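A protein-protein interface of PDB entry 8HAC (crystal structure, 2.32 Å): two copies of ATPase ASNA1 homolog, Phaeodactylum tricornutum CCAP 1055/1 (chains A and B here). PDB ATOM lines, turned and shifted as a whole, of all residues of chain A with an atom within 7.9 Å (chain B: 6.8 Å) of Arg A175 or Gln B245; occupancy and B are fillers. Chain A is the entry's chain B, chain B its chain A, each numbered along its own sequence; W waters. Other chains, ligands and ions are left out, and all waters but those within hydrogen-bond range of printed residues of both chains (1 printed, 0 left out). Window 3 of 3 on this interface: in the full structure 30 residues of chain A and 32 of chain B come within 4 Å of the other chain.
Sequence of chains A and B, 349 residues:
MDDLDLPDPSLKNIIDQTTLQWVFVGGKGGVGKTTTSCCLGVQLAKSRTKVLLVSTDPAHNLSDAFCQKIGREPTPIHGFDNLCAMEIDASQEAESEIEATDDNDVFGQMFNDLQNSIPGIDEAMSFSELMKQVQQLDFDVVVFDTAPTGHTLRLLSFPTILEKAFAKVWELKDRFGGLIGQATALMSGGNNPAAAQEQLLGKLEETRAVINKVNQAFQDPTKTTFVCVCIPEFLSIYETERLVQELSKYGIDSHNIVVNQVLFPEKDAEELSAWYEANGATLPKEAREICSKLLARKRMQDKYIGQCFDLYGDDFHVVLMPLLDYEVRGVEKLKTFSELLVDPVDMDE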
ATOM      1  N   LYS A 168     -15.294  -4.975  -8.178  1.00  0.00           N
ATOM      2  CA  LYS A 168     -16.570  -4.435  -7.729  1.00  0.00           C
ATOM      3  C   LYS A 168     -17.728  -5.049  -8.502  1.00  0.00           C
ATOM      4  O   LYS A 168     -18.745  -5.426  -7.911  1.00  0.00           O
ATOM      5  CB  LYS A 168     -16.579  -2.914  -7.872  1.00  0.00           C
ATOM      6  CG  LYS A 168     -17.779  -2.247  -7.238  1.00  0.00           C
ATOM      7  CD  LYS A 168     -17.807  -2.442  -5.725  1.00  0.00           C
ATOM      8  CE  LYS A 168     -16.711  -1.640  -5.030  1.00  0.00           C
ATOM      9  NZ  LYS A 168     -16.912  -1.609  -3.549  1.00  0.00           N
ATOM     10  N   VAL A 169     -17.600  -5.163  -9.825  1.00  0.00           N
ATOM     11  CA  VAL A 169     -18.689  -5.757 -10.601  1.00  0.00           C
ATOM     12  C   VAL A 169     -18.887  -7.224 -10.215  1.00  0.00           C
ATOM     13  O   VAL A 169     -20.023  -7.713 -10.137  1.00  0.00           O
ATOM     14  CB  VAL A 169     -18.438  -5.585 -12.111  1.00  0.00           C
ATOM     15  CG1 VAL A 169     -19.528  -6.278 -12.914  1.00  0.00           C
ATOM     16  CG2 VAL A 169     -18.391  -4.110 -12.465  1.00  0.00           C
ATOM     17  N   TRP A 170     -17.788  -7.941  -9.935  1.00  0.00           N
ATOM     18  CA  TRP A 170     -17.902  -9.345  -9.539  1.00  0.00           C
ATOM     19  C   TRP A 170     -18.580  -9.474  -8.179  1.00  0.00           C
ATOM     20  O   TRP A 170     -19.470 -10.313  -7.990  1.00  0.00           O
ATOM     21  CB  TRP A 170     -16.520 -10.000  -9.470  1.00  0.00           C
ATOM     22  CG  TRP A 170     -15.898 -10.272 -10.792  1.00  0.00           C
ATOM     23  CD1 TRP A 170     -14.757  -9.712 -11.287  1.00  0.00           C
ATOM     24  CD2 TRP A 170     -16.429 -11.083 -11.839  1.00  0.00           C
ATOM     25  NE1 TRP A 170     -14.514 -10.167 -12.556  1.00  0.00           N
ATOM     26  CE2 TRP A 170     -15.531 -11.006 -12.921  1.00  0.00           C
ATOM     27  CE3 TRP A 170     -17.563 -11.887 -11.959  1.00  0.00           C
ATOM     28  CZ2 TRP A 170     -15.734 -11.697 -14.103  1.00  0.00           C
ATOM     29  CZ3 TRP A 170     -17.761 -12.571 -13.132  1.00  0.00           C
ATOM     30  CH2 TRP A 170     -16.850 -12.472 -14.188  1.00  0.00           C
ATOM     31  N   GLU A 171     -18.168  -8.639  -7.222  1.00  0.00           N
ATOM     32  CA  GLU A 171     -18.788  -8.618  -5.903  1.00  0.00           C
ATOM     33  C   GLU A 171     -20.267  -8.287  -6.007  1.00  0.00           C
ATOM     34  O   GLU A 171     -21.100  -8.855  -5.288  1.00  0.00           O
ATOM     35  CB  GLU A 171     -18.071  -7.595  -5.021  1.00  0.00           C
ATOM     36  CG  GLU A 171     -18.870  -7.152  -3.818  1.00  0.00           C
ATOM     37  CD  GLU A 171     -18.432  -5.812  -3.253  1.00  0.00           C
ATOM     38  OE1 GLU A 171     -17.228  -5.645  -2.967  1.00  0.00           O
ATOM     39  OE2 GLU A 171     -19.301  -4.926  -3.088  1.00  0.00           O
ATOM     40  N   LEU A 172     -20.607  -7.365  -6.901  1.00  0.00           N
ATOM     41  CA  LEU A 172     -21.992  -6.974  -7.099  1.00  0.00           C
ATOM     42  C   LEU A 172     -22.822  -8.136  -7.628  1.00  0.00           C
ATOM     43  O   LEU A 172     -23.935  -8.386  -7.153  1.00  0.00           O
ATOM     44  CB  LEU A 172     -22.023  -5.788  -8.057  1.00  0.00           C
ATOM     45  CG  LEU A 172     -23.297  -5.028  -8.351  1.00  0.00           C
ATOM     46  CD1 LEU A 172     -22.857  -3.642  -8.720  1.00  0.00           C
ATOM     47  CD2 LEU A 172     -24.062  -5.686  -9.496  1.00  0.00           C
ATOM     48  N   LYS A 173     -22.301  -8.852  -8.626  1.00  0.00           N
ATOM     49  CA  LYS A 173     -23.013 -10.030  -9.115  1.00  0.00           C
ATOM     50  C   LYS A 173     -23.195 -11.053  -7.999  1.00  0.00           C
ATOM     51  O   LYS A 173     -24.304 -11.547  -7.765  1.00  0.00           O
ATOM     52  CB  LYS A 173     -22.287 -10.649 -10.311  1.00  0.00           C
ATOM     53  CG  LYS A 173     -23.125 -11.711 -11.023  1.00  0.00           C
ATOM     54  CD  LYS A 173     -22.453 -12.261 -12.278  1.00  0.00           C
ATOM     55  CE  LYS A 173     -23.150 -13.536 -12.755  1.00  0.00           C
ATOM     56  NZ  LYS A 173     -24.636 -13.438 -12.651  1.00  0.00           N
ATOM     57  N   ASP A 174     -22.116 -11.344  -7.268  1.00  0.00           N
ATOM     58  CA  ASP A 174     -22.170 -12.307  -6.173  1.00  0.00           C
ATOM     59  C   ASP A 174     -23.247 -11.944  -5.154  1.00  0.00           C
ATOM     60  O   ASP A 174     -24.049 -12.793  -4.744  1.00  0.00           O
ATOM     61  CB  ASP A 174     -20.793 -12.377  -5.506  1.00  0.00           C
ATOM     62  CG  ASP A 174     -20.781 -13.260  -4.282  1.00  0.00           C
ATOM     63  OD1 ASP A 174     -20.741 -14.502  -4.434  1.00  0.00           O
ATOM     64  OD2 ASP A 174     -20.803 -12.703  -3.165  1.00  0.00           O
ATOM     65  N   ARG A 175     -23.283 -10.673  -4.747  1.00  0.00           N
ATOM     66  CA  ARG A 175     -24.130 -10.229  -3.647  1.00  0.00           C
ATOM     67  C   ARG A 175     -25.583 -10.012  -4.058  1.00  0.00           C
ATOM     68  O   ARG A 175     -26.483 -10.208  -3.232  1.00  0.00           O
ATOM     69  CB  ARG A 175     -23.533  -8.951  -3.055  1.00  0.00           C
ATOM     70  CG  ARG A 175     -22.342  -9.196  -2.145  1.00  0.00           C
ATOM     71  CD  ARG A 175     -21.513  -7.934  -1.928  1.00  0.00           C
ATOM     72  NE  ARG A 175     -22.168  -6.845  -1.217  1.00  0.00           N
ATOM     73  CZ  ARG A 175     -22.114  -6.673   0.095  1.00  0.00           C
ATOM     74  NH1 ARG A 175     -21.486  -7.532   0.878  1.00  0.00           N
ATOM     75  NH2 ARG A 175     -22.682  -5.596   0.632  1.00  0.00           N
ATOM     76  N   PHE A 176     -25.850  -9.630  -5.315  1.00  0.00           N
ATOM     77  CA  PHE A 176     -27.215  -9.308  -5.724  1.00  0.00           C
ATOM     78  C   PHE A 176     -27.719 -10.166  -6.884  1.00  0.00           C
ATOM     79  O   PHE A 176     -28.665  -9.762  -7.575  1.00  0.00           O
ATOM     80  CB  PHE A 176     -27.314  -7.819  -6.073  1.00  0.00           C
ATOM     81  CG  PHE A 176     -26.711  -6.918  -5.030  1.00  0.00           C
ATOM     82  CD1 PHE A 176     -27.315  -6.769  -3.792  1.00  0.00           C
ATOM     83  CD2 PHE A 176     -25.532  -6.232  -5.281  1.00  0.00           C
ATOM     84  CE1 PHE A 176     -26.756  -5.946  -2.828  1.00  0.00           C
ATOM     85  CE2 PHE A 176     -24.969  -5.410  -4.320  1.00  0.00           C
ATOM     86  CZ  PHE A 176     -25.580  -5.267  -3.095  1.00  0.00           C
ATOM     87  N   GLY A 177     -27.112 -11.336  -7.114  1.00  0.00           N
ATOM     88  CA  GLY A 177     -27.600 -12.220  -8.161  1.00  0.00           C
ATOM     89  C   GLY A 177     -29.052 -12.613  -7.988  1.00  0.00           C
ATOM     90  O   GLY A 177     -29.791 -12.725  -8.966  1.00  0.00           O
ATOM     91  N   GLY A 178     -29.476 -12.845  -6.749  1.00  0.00           N
ATOM     92  CA  GLY A 178     -30.861 -13.183  -6.484  1.00  0.00           C
ATOM     93  C   GLY A 178     -31.831 -12.131  -6.980  1.00  0.00           C
ATOM     94  O   GLY A 178     -32.737 -12.429  -7.768  1.00  0.00           O
ATOM     95  N   LEU A 179     -31.642 -10.890  -6.521  1.00  0.00           N
ATOM     96  CA  LEU A 179     -32.499  -9.791  -6.954  1.00  0.00           C
ATOM     97  C   LEU A 179     -32.422  -9.590  -8.464  1.00  0.00           C
ATOM     98  O   LEU A 179     -33.448  -9.361  -9.119  1.00  0.00           O
ATOM     99  CB  LEU A 179     -32.113  -8.507  -6.216  1.00  0.00           C
ATOM    100  CG  LEU A 179     -32.862  -7.214  -6.552  1.00  0.00           C
ATOM    101  CD1 LEU A 179     -34.369  -7.427  -6.541  1.00  0.00           C
ATOM    102  CD2 LEU A 179     -32.465  -6.093  -5.599  1.00  0.00           C
ATOM    103  N   ILE A 180     -31.220  -9.688  -9.038  1.00  0.00           N
ATOM    104  CA  ILE A 180     -31.051  -9.428 -10.467  1.00  0.00           C
ATOM    105  C   ILE A 180     -31.796 -10.472 -11.294  1.00  0.00           C
ATOM    106  O   ILE A 180     -32.506 -10.140 -12.255  1.00  0.00           O
ATOM    107  CB  ILE A 180     -29.552  -9.374 -10.821  1.00  0.00           C
ATOM    108  CG1 ILE A 180     -28.945  -8.036 -10.384  1.00  0.00           C
ATOM    109  CG2 ILE A 180     -29.331  -9.610 -12.308  1.00  0.00           C
ATOM    110  CD1 ILE A 180     -27.462  -7.916 -10.663  1.00  0.00           C
ATOM    111  N   THR B 240     -31.840   0.249  -2.898  1.00  0.00           N
ATOM    112  CA  THR B 240     -32.183   0.019  -1.498  1.00  0.00           C
ATOM    113  C   THR B 240     -31.479  -1.215  -0.957  1.00  0.00           C
ATOM    114  O   THR B 240     -30.995  -1.211   0.177  1.00  0.00           O
ATOM    115  CB  THR B 240     -33.697  -0.123  -1.346  1.00  0.00           C
ATOM    116  OG1 THR B 240     -34.325   1.148  -1.570  1.00  0.00           O
ATOM    117  CG2 THR B 240     -34.060  -0.655   0.034  1.00  0.00           C
ATOM    118  N   GLU B 241     -31.413  -2.280  -1.756  1.00  0.00           N
ATOM    119  CA  GLU B 241     -30.727  -3.495  -1.322  1.00  0.00           C
ATOM    120  C   GLU B 241     -29.224  -3.265  -1.189  1.00  0.00           C
ATOM    121  O   GLU B 241     -28.600  -3.738  -0.227  1.00  0.00           O
ATOM    122  CB  GLU B 241     -31.018  -4.635  -2.296  1.00  0.00           C
ATOM    123  CG  GLU B 241     -30.361  -5.959  -1.946  1.00  0.00           C
ATOM    124  CD  GLU B 241     -30.837  -6.540  -0.622  1.00  0.00           C
ATOM    125  OE1 GLU B 241     -31.879  -6.090  -0.097  1.00  0.00           O
ATOM    126  OE2 GLU B 241     -30.170  -7.467  -0.114  1.00  0.00           O
ATOM    127  N   ARG B 242     -28.631  -2.539  -2.143  1.00  0.00           N
ATOM    128  CA  ARG B 242     -27.230  -2.136  -2.010  1.00  0.00           C
ATOM    129  C   ARG B 242     -26.996  -1.385  -0.705  1.00  0.00           C
ATOM    130  O   ARG B 242     -26.044  -1.671   0.034  1.00  0.00           O
ATOM    131  CB  ARG B 242     -26.810  -1.266  -3.191  1.00  0.00           C
ATOM    132  CG  ARG B 242     -26.643  -1.989  -4.505  1.00  0.00           C
ATOM    133  CD  ARG B 242     -26.102  -1.031  -5.553  1.00  0.00           C
ATOM    134  NE  ARG B 242     -24.693  -0.725  -5.337  1.00  0.00           N
ATOM    135  CZ  ARG B 242     -24.148   0.473  -5.503  1.00  0.00           C
ATOM    136  NH1 ARG B 242     -24.871   1.517  -5.870  1.00  0.00           N
ATOM    137  NH2 ARG B 242     -22.845   0.629  -5.291  1.00  0.00           N
ATOM    138  N   LEU B 243     -27.855  -0.403  -0.416  1.00  0.00           N
ATOM    139  CA  LEU B 243     -27.672   0.410   0.781  1.00  0.00           C
ATOM    140  C   LEU B 243     -27.834  -0.423   2.045  1.00  0.00           C
ATOM    141  O   LEU B 243     -27.053  -0.280   2.995  1.00  0.00           O
ATOM    142  CB  LEU B 243     -28.654   1.582   0.774  1.00  0.00           C
ATOM    143  CG  LEU B 243     -28.682   2.415   2.058  1.00  0.00           C
ATOM    144  CD1 LEU B 243     -27.329   3.066   2.303  1.00  0.00           C
ATOM    145  CD2 LEU B 243     -29.794   3.450   2.001  1.00  0.00           C
ATOM    146  N   VAL B 244     -28.840  -1.305   2.070  1.00  0.00           N
ATOM    147  CA  VAL B 244     -29.095  -2.129   3.249  1.00  0.00           C
ATOM    148  C   VAL B 244     -27.907  -3.042   3.532  1.00  0.00           C
ATOM    149  O   VAL B 244     -27.446  -3.162   4.678  1.00  0.00           O
ATOM    150  CB  VAL B 244     -30.390  -2.940   3.063  1.00  0.00           C
ATOM    151  CG1 VAL B 244     -30.434  -4.109   4.037  1.00  0.00           C
ATOM    152  CG2 VAL B 244     -31.605  -2.053   3.249  1.00  0.00           C
ATOM    153  N   GLN B 245     -27.389  -3.699   2.488  1.00  0.00           N
ATOM    154  CA  GLN B 245     -26.241  -4.582   2.684  1.00  0.00           C
ATOM    155  C   GLN B 245     -24.998  -3.802   3.107  1.00  0.00           C
ATOM    156  O   GLN B 245     -24.218  -4.282   3.937  1.00  0.00           O
ATOM    157  CB  GLN B 245     -25.975  -5.387   1.416  1.00  0.00           C
ATOM    158  CG  GLN B 245     -26.977  -6.508   1.193  1.00  0.00           C
ATOM    159  CD  GLN B 245     -26.560  -7.449   0.079  1.00  0.00           C
ATOM    160  OE1 GLN B 245     -25.376  -7.558  -0.245  1.00  0.00           O
ATOM    161  NE2 GLN B 245     -27.536  -8.126  -0.520  1.00  0.00           N
ATOM    162  N   GLU B 246     -24.797  -2.596   2.557  1.00  0.00           N
ATOM    163  CA  GLU B 246     -23.640  -1.798   2.958  1.00  0.00           C
ATOM    164  C   GLU B 246     -23.739  -1.373   4.420  1.00  0.00           C
ATOM    165  O   GLU B 246     -22.741  -1.406   5.152  1.00  0.00           O
ATOM    166  CB  GLU B 246     -23.500  -0.576   2.052  1.00  0.00           C
ATOM    167  CG  GLU B 246     -22.105   0.051   2.053  1.00  0.00           C
ATOM    168  CD  GLU B 246     -21.068  -0.779   1.308  1.00  0.00           C
ATOM    169  OE1 GLU B 246     -21.410  -1.871   0.801  1.00  0.00           O
ATOM    170  OE2 GLU B 246     -19.900  -0.337   1.230  1.00  0.00           O
ATOM    171  N   LEU B 247     -24.929  -0.961   4.860  1.00  0.00           N
ATOM    172  CA  LEU B 247     -25.123  -0.630   6.268  1.00  0.00           C
ATOM    173  C   LEU B 247     -24.877  -1.844   7.153  1.00  0.00           C
ATOM    174  O   LEU B 247     -24.341  -1.719   8.262  1.00  0.00           O
ATOM    175  CB  LEU B 247     -26.536  -0.096   6.492  1.00  0.00           C
ATOM    176  CG  LEU B 247     -26.893   1.229   5.825  1.00  0.00           C
ATOM    177  CD1 LEU B 247     -28.404   1.432   5.845  1.00  0.00           C
ATOM    178  CD2 LEU B 247     -26.171   2.376   6.520  1.00  0.00           C
ATOM    179  N   SER B 248     -25.287  -3.029   6.692  1.00  0.00           N
ATOM    180  CA  SER B 248     -25.045  -4.234   7.483  1.00  0.00           C
ATOM    181  C   SER B 248     -23.554  -4.539   7.588  1.00  0.00           C
ATOM    182  O   SER B 248     -23.065  -4.908   8.663  1.00  0.00           O
ATOM    183  CB  SER B 248     -25.796  -5.422   6.882  1.00  0.00           C
ATOM    184  OG  SER B 248     -25.763  -6.528   7.762  1.00  0.00           O
ATOM    185  N   LYS B 249     -22.815  -4.380   6.487  1.00  0.00           N
ATOM    186  CA  LYS B 249     -21.374  -4.600   6.532  1.00  0.00           C
ATOM    187  C   LYS B 249     -20.707  -3.710   7.575  1.00  0.00           C
ATOM    188  O   LYS B 249     -19.826  -4.160   8.317  1.00  0.00           O
ATOM    189  CB  LYS B 249     -20.754  -4.343   5.161  1.00  0.00           C
ATOM    190  CG  LYS B 249     -19.242  -4.221   5.217  1.00  0.00           C
ATOM    191  CD  LYS B 249     -18.622  -4.060   3.847  1.00  0.00           C
ATOM    192  CE  LYS B 249     -17.106  -4.086   3.947  1.00  0.00           C
ATOM    193  NZ  LYS B 249     -16.455  -3.378   2.813  1.00  0.00           N
ATOM    194  N   TYR B 250     -21.123  -2.448   7.656  1.00  0.00           N
ATOM    195  CA  TYR B 250     -20.498  -1.480   8.543  1.00  0.00           C
ATOM    196  C   TYR B 250     -21.180  -1.386   9.897  1.00  0.00           C
ATOM    197  O   TYR B 250     -20.961  -0.408  10.621  1.00  0.00           O
ATOM    198  CB  TYR B 250     -20.451  -0.109   7.870  1.00  0.00           C
ATOM    199  CG  TYR B 250     -19.426  -0.051   6.768  1.00  0.00           C
ATOM    200  CD1 TYR B 250     -18.071   0.030   7.063  1.00  0.00           C
ATOM    201  CD2 TYR B 250     -19.805  -0.092   5.435  1.00  0.00           C
ATOM    202  CE1 TYR B 250     -17.122   0.076   6.062  1.00  0.00           C
ATOM    203  CE2 TYR B 250     -18.861  -0.042   4.425  1.00  0.00           C
ATOM    204  CZ  TYR B 250     -17.521   0.042   4.746  1.00  0.00           C
ATOM    205  OH  TYR B 250     -16.580   0.091   3.742  1.00  0.00           O
HETATM  206  O   HOH W   1     -23.591  -2.844  -0.769  1.00  0.00           O
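The side-chain amide oxygen of Gln B245 sits close to the guanidinium group of Arg A175 (3.4 Å). NH2 of Arg A175 is in salt-bridge range of OE1 of Glu B246 (3.9 Å).
OE2 of Glu B241 lies within hydrogen-bond range of NE2 of Gln B245 (2.7 Å). The guanidinium group (NE) of Arg A175 lies within salt-bridge range of the side-chain carboxylate (OE2) of Glu A171, 3.9 Å away.
Among the printed residues, pairs that only touch across the chains: Phe A176 with Gln B245, Phe A176 with Glu B241, Phe A176 with Arg B242 and Leu A179 with Glu B241.
Arg A175 touches just these residues of chain B: Gln B245 and Glu B246. Gln B245 touches just these residues of chain A: Arg A175 and Phe A176. Of the printed residues of chain A, Arg B242 touches Phe A176 (3.7 Å). Printed residues of chain B within 4 Å of Phe A176: Glu B241, Arg B242 and Gln B245. Printed residues of chain A within 4 Å of Glu B246: Arg A175 (3.9 Å). Of the printed residues of chain B, Leu A179 touches Glu B241 (3.9 Å). Leu B243 touches none of the printed residues of chain A. Leu B247 touches none of the printed residues of chain A. The nearest residue of chain B that does not touch Arg A175 is Lys B249 (5.1 Å).
Printed residues of chain B that touch a printed residue of chain A: Glu B241, Arg B242, Gln B245 and Glu B246. Of the 13 printed residues of chain A, 3 touch a printed residue of chain B. Hydrophobic or aromatic side chains of chain A that line the printed part of chain B: Phe A176 and Leu A179. Among the printed residues, 6 pairs touch across the chains.
No position is printed for both chains.
Water W1 lies within hydrogen-bond range of O of Arg B242 (2.8 Å), OE1 of Glu B246 (2.9 Å) and NH2 of Arg A175 (3.2 Å).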
